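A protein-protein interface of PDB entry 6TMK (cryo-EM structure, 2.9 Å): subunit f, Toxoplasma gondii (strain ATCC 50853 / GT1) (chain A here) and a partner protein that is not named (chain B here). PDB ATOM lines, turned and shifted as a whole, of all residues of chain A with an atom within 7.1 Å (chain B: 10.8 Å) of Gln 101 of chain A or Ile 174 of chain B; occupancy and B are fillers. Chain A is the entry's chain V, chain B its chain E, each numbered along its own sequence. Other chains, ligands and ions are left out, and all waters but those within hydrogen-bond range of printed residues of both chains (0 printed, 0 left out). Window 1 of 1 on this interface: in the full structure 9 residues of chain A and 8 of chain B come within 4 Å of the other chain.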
ATOM      1  N   LYS A  89     -18.352 -23.384   1.376  1.00  0.00           N
ATOM      2  CA  LYS A  89     -17.717 -22.201   1.938  1.00  0.00           C
ATOM      3  C   LYS A  89     -17.348 -21.214   0.842  1.00  0.00           C
ATOM      4  O   LYS A  89     -17.624 -20.008   0.939  1.00  0.00           O
ATOM      5  CB  LYS A  89     -16.484 -22.611   2.728  1.00  0.00           C
ATOM      6  CG  LYS A  89     -15.984 -21.568   3.665  1.00  0.00           C
ATOM      7  CD  LYS A  89     -14.637 -21.938   4.196  1.00  0.00           C
ATOM      8  CE  LYS A  89     -14.139 -20.932   5.185  1.00  0.00           C
ATOM      9  NZ  LYS A  89     -13.590 -21.568   6.394  1.00  0.00           N
ATOM     10  N   THR A  91     -18.600 -21.008  -2.188  1.00  0.00           N
ATOM     11  CA  THR A  91     -19.816 -20.485  -2.798  1.00  0.00           C
ATOM     12  C   THR A  91     -20.476 -19.449  -1.901  1.00  0.00           C
ATOM     13  O   THR A  91     -21.038 -18.464  -2.388  1.00  0.00           O
ATOM     14  CB  THR A  91     -20.776 -21.633  -3.107  1.00  0.00           C
ATOM     15  OG1 THR A  91     -20.066 -22.683  -3.764  1.00  0.00           O
ATOM     16  CG2 THR A  91     -21.907 -21.168  -3.978  1.00  0.00           C
ATOM     17  N   ALA A  92     -20.405 -19.647  -0.589  1.00  0.00           N
ATOM     18  CA  ALA A  92     -20.972 -18.689   0.346  1.00  0.00           C
ATOM     19  C   ALA A  92     -20.256 -17.355   0.236  1.00  0.00           C
ATOM     20  O   ALA A  92     -20.893 -16.300   0.166  1.00  0.00           O
ATOM     21  CB  ALA A  92     -20.891 -19.243   1.764  1.00  0.00           C
ATOM     22  N   GLN A  93     -18.925 -17.384   0.226  1.00  0.00           N
ATOM     23  CA  GLN A  93     -18.166 -16.143   0.113  1.00  0.00           C
ATOM     24  C   GLN A  93     -18.422 -15.472  -1.232  1.00  0.00           C
ATOM     25  O   GLN A  93     -18.523 -14.242  -1.317  1.00  0.00           O
ATOM     26  CB  GLN A  93     -16.686 -16.412   0.322  1.00  0.00           C
ATOM     27  CG  GLN A  93     -16.356 -16.876   1.695  1.00  0.00           C
ATOM     28  CD  GLN A  93     -14.883 -16.884   1.974  1.00  0.00           C
ATOM     29  OE1 GLN A  93     -14.300 -15.873   2.354  1.00  0.00           O
ATOM     30  NE2 GLN A  93     -14.268 -18.036   1.796  1.00  0.00           N
ATOM     31  N   LEU A  94     -18.545 -16.269  -2.289  1.00  0.00           N
ATOM     32  CA  LEU A  94     -18.849 -15.738  -3.610  1.00  0.00           C
ATOM     33  C   LEU A  94     -20.185 -15.007  -3.616  1.00  0.00           C
ATOM     34  O   LEU A  94     -20.290 -13.870  -4.094  1.00  0.00           O
ATOM     35  CB  LEU A  94     -18.883 -16.894  -4.598  1.00  0.00           C
ATOM     36  CG  LEU A  94     -19.152 -16.655  -6.075  1.00  0.00           C
ATOM     37  CD1 LEU A  94     -18.041 -15.882  -6.706  1.00  0.00           C
ATOM     38  CD2 LEU A  94     -19.366 -17.964  -6.746  1.00  0.00           C
ATOM     39  N   VAL A  95     -21.227 -15.663  -3.108  1.00  0.00           N
ATOM     40  CA  VAL A  95     -22.551 -15.063  -3.104  1.00  0.00           C
ATOM     41  C   VAL A  95     -22.574 -13.829  -2.216  1.00  0.00           C
ATOM     42  O   VAL A  95     -23.226 -12.831  -2.534  1.00  0.00           O
ATOM     43  CB  VAL A  95     -23.596 -16.103  -2.662  1.00  0.00           C
ATOM     44  CG1 VAL A  95     -24.928 -15.452  -2.437  1.00  0.00           C
ATOM     45  CG2 VAL A  95     -23.713 -17.200  -3.682  1.00  0.00           C
ATOM     46  N   ALA A  96     -21.855 -13.866  -1.097  1.00  0.00           N
ATOM     47  CA  ALA A  96     -21.857 -12.721  -0.205  1.00  0.00           C
ATOM     48  C   ALA A  96     -21.130 -11.530  -0.811  1.00  0.00           C
ATOM     49  O   ALA A  96     -21.496 -10.383  -0.542  1.00  0.00           O
ATOM     50  CB  ALA A  96     -21.249 -13.106   1.135  1.00  0.00           C
ATOM     51  N   ALA A  97     -20.111 -11.776  -1.631  1.00  0.00           N
ATOM     52  CA  ALA A  97     -19.439 -10.680  -2.314  1.00  0.00           C
ATOM     53  C   ALA A  97     -20.226 -10.156  -3.510  1.00  0.00           C
ATOM     54  O   ALA A  97     -20.112  -8.973  -3.843  1.00  0.00           O
ATOM     55  CB  ALA A  97     -18.046 -11.117  -2.753  1.00  0.00           C
ATOM     56  N   TYR A  99     -23.835 -10.528  -4.138  1.00  0.00           N
ATOM     57  CA  TYR A  99     -25.196 -10.100  -3.858  1.00  0.00           C
ATOM     58  C   TYR A  99     -25.446  -9.777  -2.403  1.00  0.00           C
ATOM     59  O   TYR A  99     -26.411  -9.063  -2.111  1.00  0.00           O
ATOM     60  CB  TYR A  99     -26.203 -11.181  -4.269  1.00  0.00           C
ATOM     61  CG  TYR A  99     -26.038 -11.758  -5.643  1.00  0.00           C
ATOM     62  CD1 TYR A  99     -26.547 -11.114  -6.746  1.00  0.00           C
ATOM     63  CD2 TYR A  99     -25.405 -12.966  -5.834  1.00  0.00           C
ATOM     64  CE1 TYR A  99     -26.408 -11.642  -7.995  1.00  0.00           C
ATOM     65  CE2 TYR A  99     -25.266 -13.497  -7.076  1.00  0.00           C
ATOM     66  CZ  TYR A  99     -25.772 -12.838  -8.157  1.00  0.00           C
ATOM     67  OH  TYR A  99     -25.633 -13.375  -9.409  1.00  0.00           O
ATOM     68  N   GLY A 100     -24.647 -10.292  -1.490  1.00  0.00           N
ATOM     69  CA  GLY A 100     -24.953 -10.295  -0.082  1.00  0.00           C
ATOM     70  C   GLY A 100     -25.368 -11.673   0.397  1.00  0.00           C
ATOM     71  O   GLY A 100     -25.761 -12.546  -0.377  1.00  0.00           O
ATOM     72  N   GLN A 101     -25.277 -11.858   1.705  1.00  0.00           N
ATOM     73  CA  GLN A 101     -25.594 -13.145   2.299  1.00  0.00           C
ATOM     74  C   GLN A 101     -27.065 -13.466   2.088  1.00  0.00           C
ATOM     75  O   GLN A 101     -27.945 -12.690   2.473  1.00  0.00           O
ATOM     76  CB  GLN A 101     -25.246 -13.109   3.783  1.00  0.00           C
ATOM     77  CG  GLN A 101     -25.432 -14.395   4.537  1.00  0.00           C
ATOM     78  CD  GLN A 101     -24.662 -15.545   3.966  1.00  0.00           C
ATOM     79  OE1 GLN A 101     -23.546 -15.392   3.474  1.00  0.00           O
ATOM     80  NE2 GLN A 101     -25.262 -16.714   4.020  1.00  0.00           N
ATOM     81  N   GLY A 102     -27.326 -14.610   1.466  1.00  0.00           N
ATOM     82  CA  GLY A 102     -28.669 -14.992   1.105  1.00  0.00           C
ATOM     83  C   GLY A 102     -29.131 -14.453  -0.225  1.00  0.00           C
ATOM     84  O   GLY A 102     -30.328 -14.527  -0.520  1.00  0.00           O
ATOM     85  N   GLY A 103     -28.220 -13.921  -1.041  1.00  0.00           N
ATOM     86  CA  GLY A 103     -28.594 -13.290  -2.286  1.00  0.00           C
ATOM     87  C   GLY A 103     -29.197 -14.224  -3.309  1.00  0.00           C
ATOM     88  O   GLY A 103     -29.927 -13.767  -4.192  1.00  0.00           O
ATOM     89  N   GLN A 104     -28.906 -15.519  -3.219  1.00  0.00           N
ATOM     90  CA  GLN A 104     -29.422 -16.457  -4.200  1.00  0.00           C
ATOM     91  C   GLN A 104     -30.853 -16.862  -3.895  1.00  0.00           C
ATOM     92  O   GLN A 104     -31.532 -17.402  -4.772  1.00  0.00           O
ATOM     93  CB  GLN A 104     -28.515 -17.687  -4.305  1.00  0.00           C
ATOM     94  CG  GLN A 104     -28.569 -18.686  -3.171  1.00  0.00           C
ATOM     95  CD  GLN A 104     -27.799 -18.237  -1.958  1.00  0.00           C
ATOM     96  OE1 GLN A 104     -27.612 -17.049  -1.732  1.00  0.00           O
ATOM     97  NE2 GLN A 104     -27.311 -19.189  -1.194  1.00  0.00           N
ATOM     98  N   LEU A 106     -33.151 -14.583  -2.780  1.00  0.00           N
ATOM     99  CA  LEU A 106     -33.972 -13.387  -2.743  1.00  0.00           C
ATOM    100  C   LEU A 106     -35.198 -13.543  -3.624  1.00  0.00           C
ATOM    101  O   LEU A 106     -35.195 -14.275  -4.616  1.00  0.00           O
ATOM    102  CB  LEU A 106     -33.182 -12.164  -3.188  1.00  0.00           C
ATOM    103  CG  LEU A 106     -32.047 -11.722  -2.276  1.00  0.00           C
ATOM    104  CD1 LEU A 106     -31.215 -10.671  -2.952  1.00  0.00           C
ATOM    105  CD2 LEU A 106     -32.581 -11.208  -0.979  1.00  0.00           C
ATOM    106  N   GLY B 168     -14.227  -0.882   5.237  1.00  0.00           N
ATOM    107  CA  GLY B 168     -15.047  -1.208   6.375  1.00  0.00           C
ATOM    108  C   GLY B 168     -14.853  -2.630   6.838  1.00  0.00           C
ATOM    109  O   GLY B 168     -14.317  -3.477   6.129  1.00  0.00           O
ATOM    110  N   MET B 169     -15.308  -2.882   8.053  1.00  0.00           N
ATOM    111  CA  MET B 169     -15.198  -4.198   8.656  1.00  0.00           C
ATOM    112  C   MET B 169     -16.393  -5.062   8.297  1.00  0.00           C
ATOM    113  O   MET B 169     -17.436  -4.583   7.853  1.00  0.00           O
ATOM    114  CB  MET B 169     -15.093  -4.102  10.176  1.00  0.00           C
ATOM    115  CG  MET B 169     -13.774  -3.570  10.696  1.00  0.00           C
ATOM    116  SD  MET B 169     -13.459  -4.035  12.406  1.00  0.00           S
ATOM    117  CE  MET B 169     -14.882  -3.319  13.216  1.00  0.00           C
ATOM    118  N   GLN B 170     -16.215  -6.361   8.481  1.00  0.00           N
ATOM    119  CA  GLN B 170     -17.292  -7.301   8.248  1.00  0.00           C
ATOM    120  C   GLN B 170     -18.340  -7.103   9.333  1.00  0.00           C
ATOM    121  O   GLN B 170     -18.073  -7.310  10.520  1.00  0.00           O
ATOM    122  CB  GLN B 170     -16.756  -8.720   8.242  1.00  0.00           C
ATOM    123  CG  GLN B 170     -17.557  -9.673   7.409  1.00  0.00           C
ATOM    124  CD  GLN B 170     -17.203 -11.109   7.687  1.00  0.00           C
ATOM    125  OE1 GLN B 170     -16.034 -11.480   7.703  1.00  0.00           O
ATOM    126  NE2 GLN B 170     -18.210 -11.920   7.941  1.00  0.00           N
ATOM    127  N   TYR B 171     -19.531  -6.699   8.915  1.00  0.00           N
ATOM    128  CA  TYR B 171     -20.612  -6.298   9.798  1.00  0.00           C
ATOM    129  C   TYR B 171     -21.626  -7.402  10.017  1.00  0.00           C
ATOM    130  O   TYR B 171     -22.210  -7.491  11.098  1.00  0.00           O
ATOM    131  CB  TYR B 171     -21.289  -5.055   9.217  1.00  0.00           C
ATOM    132  CG  TYR B 171     -21.978  -4.158  10.200  1.00  0.00           C
ATOM    133  CD1 TYR B 171     -23.358  -4.103  10.269  1.00  0.00           C
ATOM    134  CD2 TYR B 171     -21.246  -3.345  11.044  1.00  0.00           C
ATOM    135  CE1 TYR B 171     -23.994  -3.273  11.157  1.00  0.00           C
ATOM    136  CE2 TYR B 171     -21.873  -2.505  11.941  1.00  0.00           C
ATOM    137  CZ  TYR B 171     -23.249  -2.478  11.994  1.00  0.00           C
ATOM    138  OH  TYR B 171     -23.877  -1.641  12.885  1.00  0.00           O
ATOM    139  N   SER B 172     -21.848  -8.233   9.009  1.00  0.00           N
ATOM    140  CA  SER B 172     -22.750  -9.366   9.071  1.00  0.00           C
ATOM    141  C   SER B 172     -21.947 -10.634   8.825  1.00  0.00           C
ATOM    142  O   SER B 172     -20.867 -10.605   8.233  1.00  0.00           O
ATOM    143  CB  SER B 172     -23.887  -9.236   8.049  1.00  0.00           C
ATOM    144  OG  SER B 172     -24.755  -8.171   8.374  1.00  0.00           O
ATOM    145  N   SER B 173     -22.487 -11.750   9.287  1.00  0.00           N
ATOM    146  CA  SER B 173     -21.813 -13.026   9.145  1.00  0.00           C
ATOM    147  C   SER B 173     -22.069 -13.630   7.769  1.00  0.00           C
ATOM    148  O   SER B 173     -23.066 -13.344   7.103  1.00  0.00           O
ATOM    149  CB  SER B 173     -22.258 -13.984  10.246  1.00  0.00           C
ATOM    150  OG  SER B 173     -22.241 -13.355  11.508  1.00  0.00           O
ATOM    151  N   ILE B 174     -21.145 -14.489   7.353  1.00  0.00           N
ATOM    152  CA  ILE B 174     -21.239 -15.222   6.100  1.00  0.00           C
ATOM    153  C   ILE B 174     -21.358 -16.696   6.440  1.00  0.00           C
ATOM    154  O   ILE B 174     -20.600 -17.210   7.268  1.00  0.00           O
ATOM    155  CB  ILE B 174     -20.012 -14.972   5.205  1.00  0.00           C
ATOM    156  CG1 ILE B 174     -19.995 -13.540   4.693  1.00  0.00           C
ATOM    157  CG2 ILE B 174     -20.023 -15.901   4.014  1.00  0.00           C
ATOM    158  CD1 ILE B 174     -18.623 -13.022   4.460  1.00  0.00           C
ATOM    159  N   TYR B 175     -22.303 -17.373   5.802  1.00  0.00           N
ATOM    160  CA  TYR B 175     -22.582 -18.755   6.144  1.00  0.00           C
ATOM    161  C   TYR B 175     -23.311 -19.436   5.000  1.00  0.00           C
ATOM    162  O   TYR B 175     -23.820 -18.796   4.079  1.00  0.00           O
ATOM    163  CB  TYR B 175     -23.388 -18.854   7.442  1.00  0.00           C
ATOM    164  CG  TYR B 175     -24.699 -18.115   7.433  1.00  0.00           C
ATOM    165  CD1 TYR B 175     -25.847 -18.707   6.956  1.00  0.00           C
ATOM    166  CD2 TYR B 175     -24.786 -16.825   7.912  1.00  0.00           C
ATOM    167  CE1 TYR B 175     -27.033 -18.039   6.948  1.00  0.00           C
ATOM    168  CE2 TYR B 175     -25.967 -16.152   7.909  1.00  0.00           C
ATOM    169  CZ  TYR B 175     -27.092 -16.760   7.426  1.00  0.00           C
ATOM    170  OH  TYR B 175     -28.279 -16.079   7.426  1.00  0.00           O
ATOM    171  N   TRP B 176     -23.340 -20.760   5.080  1.00  0.00           N
ATOM    172  CA  TRP B 176     -24.058 -21.608   4.144  1.00  0.00           C
ATOM    173  C   TRP B 176     -24.966 -22.516   4.947  1.00  0.00           C
ATOM    174  O   TRP B 176     -24.497 -23.254   5.818  1.00  0.00           O
ATOM    175  CB  TRP B 176     -23.098 -22.435   3.294  1.00  0.00           C
ATOM    176  CG  TRP B 176     -23.703 -22.983   2.053  1.00  0.00           C
ATOM    177  CD1 TRP B 176     -24.147 -24.249   1.852  1.00  0.00           C
ATOM    178  CD2 TRP B 176     -23.935 -22.280   0.836  1.00  0.00           C
ATOM    179  NE1 TRP B 176     -24.638 -24.381   0.586  1.00  0.00           N
ATOM    180  CE2 TRP B 176     -24.522 -23.183  -0.061  1.00  0.00           C
ATOM    181  CE3 TRP B 176     -23.706 -20.973   0.418  1.00  0.00           C
ATOM    182  CZ2 TRP B 176     -24.875 -22.823  -1.345  1.00  0.00           C
ATOM    183  CZ3 TRP B 176     -24.057 -20.620  -0.850  1.00  0.00           C
ATOM    184  CH2 TRP B 176     -24.637 -21.537  -1.721  1.00  0.00           C
ATOM    185  N   GLU B 177     -26.258 -22.448   4.670  1.00  0.00           N
ATOM    186  CA  GLU B 177     -27.208 -23.280   5.383  1.00  0.00           C
ATOM    187  C   GLU B 177     -27.060 -24.735   4.972  1.00  0.00           C
ATOM    188  O   GLU B 177     -26.600 -25.056   3.877  1.00  0.00           O
ATOM    189  CB  GLU B 177     -28.634 -22.800   5.137  1.00  0.00           C
ATOM    190  CG  GLU B 177     -28.956 -21.501   5.831  1.00  0.00           C
ATOM    191  CD  GLU B 177     -30.405 -21.091   5.693  1.00  0.00           C
ATOM    192  OE1 GLU B 177     -31.276 -21.979   5.597  1.00  0.00           O
ATOM    193  OE2 GLU B 177     -30.676 -19.873   5.697  1.00  0.00           O
ATOM    194  N   THR B 178     -27.466 -25.614   5.875  1.00  0.00           N
ATOM    195  CA  THR B 178     -27.250 -27.037   5.692  1.00  0.00           C
ATOM    196  C   THR B 178     -28.005 -27.522   4.464  1.00  0.00           C
ATOM    197  O   THR B 178     -29.198 -27.254   4.300  1.00  0.00           O
ATOM    198  CB  THR B 178     -27.694 -27.789   6.942  1.00  0.00           C
ATOM    199  OG1 THR B 178     -27.069 -27.208   8.089  1.00  0.00           O
ATOM    200  CG2 THR B 178     -27.305 -29.241   6.864  1.00  0.00           C
ATOM    201  N   HIS B 180     -28.030 -26.721   1.393  1.00  0.00           N
ATOM    202  CA  HIS B 180     -28.337 -25.851   0.270  1.00  0.00           C
ATOM    203  C   HIS B 180     -27.401 -26.158  -0.887  1.00  0.00           C
ATOM    204  O   HIS B 180     -26.204 -26.382  -0.697  1.00  0.00           O
ATOM    205  CB  HIS B 180     -28.204 -24.383   0.661  1.00  0.00           C
ATOM    206  CG  HIS B 180     -29.395 -23.826   1.368  1.00  0.00           C
ATOM    207  ND1 HIS B 180     -29.519 -22.486   1.656  1.00  0.00           N
ATOM    208  CD2 HIS B 180     -30.512 -24.420   1.848  1.00  0.00           C
ATOM    209  CE1 HIS B 180     -30.662 -22.277   2.280  1.00  0.00           C
ATOM    210  NE2 HIS B 180     -31.283 -23.434   2.411  1.00  0.00           N
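O of Tyr 175 of chain B lies within hydrogen-bond range of NE2 of Gln 101 of chain A (2.5 Å).
O of His 180 of chain B is in hydrogen-bond range of NE1 of Trp 176 of chain B, 2.8 Å away.
Among the printed residues, merely in contact across the chains: Gln 101 of chain A with Ile 174 of chain B (3.5 Å), Thr 91 of chain A with Trp 176 of chain B (3.6 Å), Ala 92 of chain A with Trp 176 of chain B (3.6 Å), Gln 104 of chain A with Trp 176 of chain B (3.6 Å), Gln 101 of chain A with Ser 173 of chain B (3.6 Å), Ala 92 of chain A with Tyr 175 of chain B (3.8 Å), Ala 96 of chain A with Ile 174 of chain B (3.8 Å) and Ala 92 of chain A with Ile 174 of chain B (3.97 Å).
Of chain B, only Ser 173, Ile 174 and Tyr 175 come within 4 Å of Gln 101 of chain A.
Ile 174 of chain B touches just these residues of chain A: Ala 92 (3.97 Å), Ala 96 (3.8 Å) and Gln 101 (3.5 Å).
Ala 92 of chain A touches just these residues of chain B: Ile 174, Tyr 175 and Trp 176.
Ala 96 of chain A touches one residue of chain B.
No residue of chain B comes within 4 Å of Gly 100 of chain A.
No residue of chain B comes within 4 Å of Gly 102 of chain A.
Of the printed residues of chain B, Gln 104 of chain A touches Trp 176.
Of the printed residues of chain A, Trp 176 of chain B touches Thr 91, Ala 92 and Gln 104.
The nearest printed residue of chain B that does not touch Gln 104 of chain A is His 180 of chain B (4.9 Å).
Hydrophobic or aromatic side chains of chain A within 4 Å of the printed part of chain B: Ala 92 and Ala 96.
Along chain A the printed residues that touch a printed residue of chain B span positions 91 to 104.
Printed residues of chain B that touch a printed residue of chain A: Ser 173, Ile 174, Tyr 175 and Trp 176.
Among the printed residues, 9 pairs touch across the chains.
Among the printed residues, no Asp or Glu carboxylate lies within 4 Å of a Lys or Arg side-chain nitrogen of the other chain.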
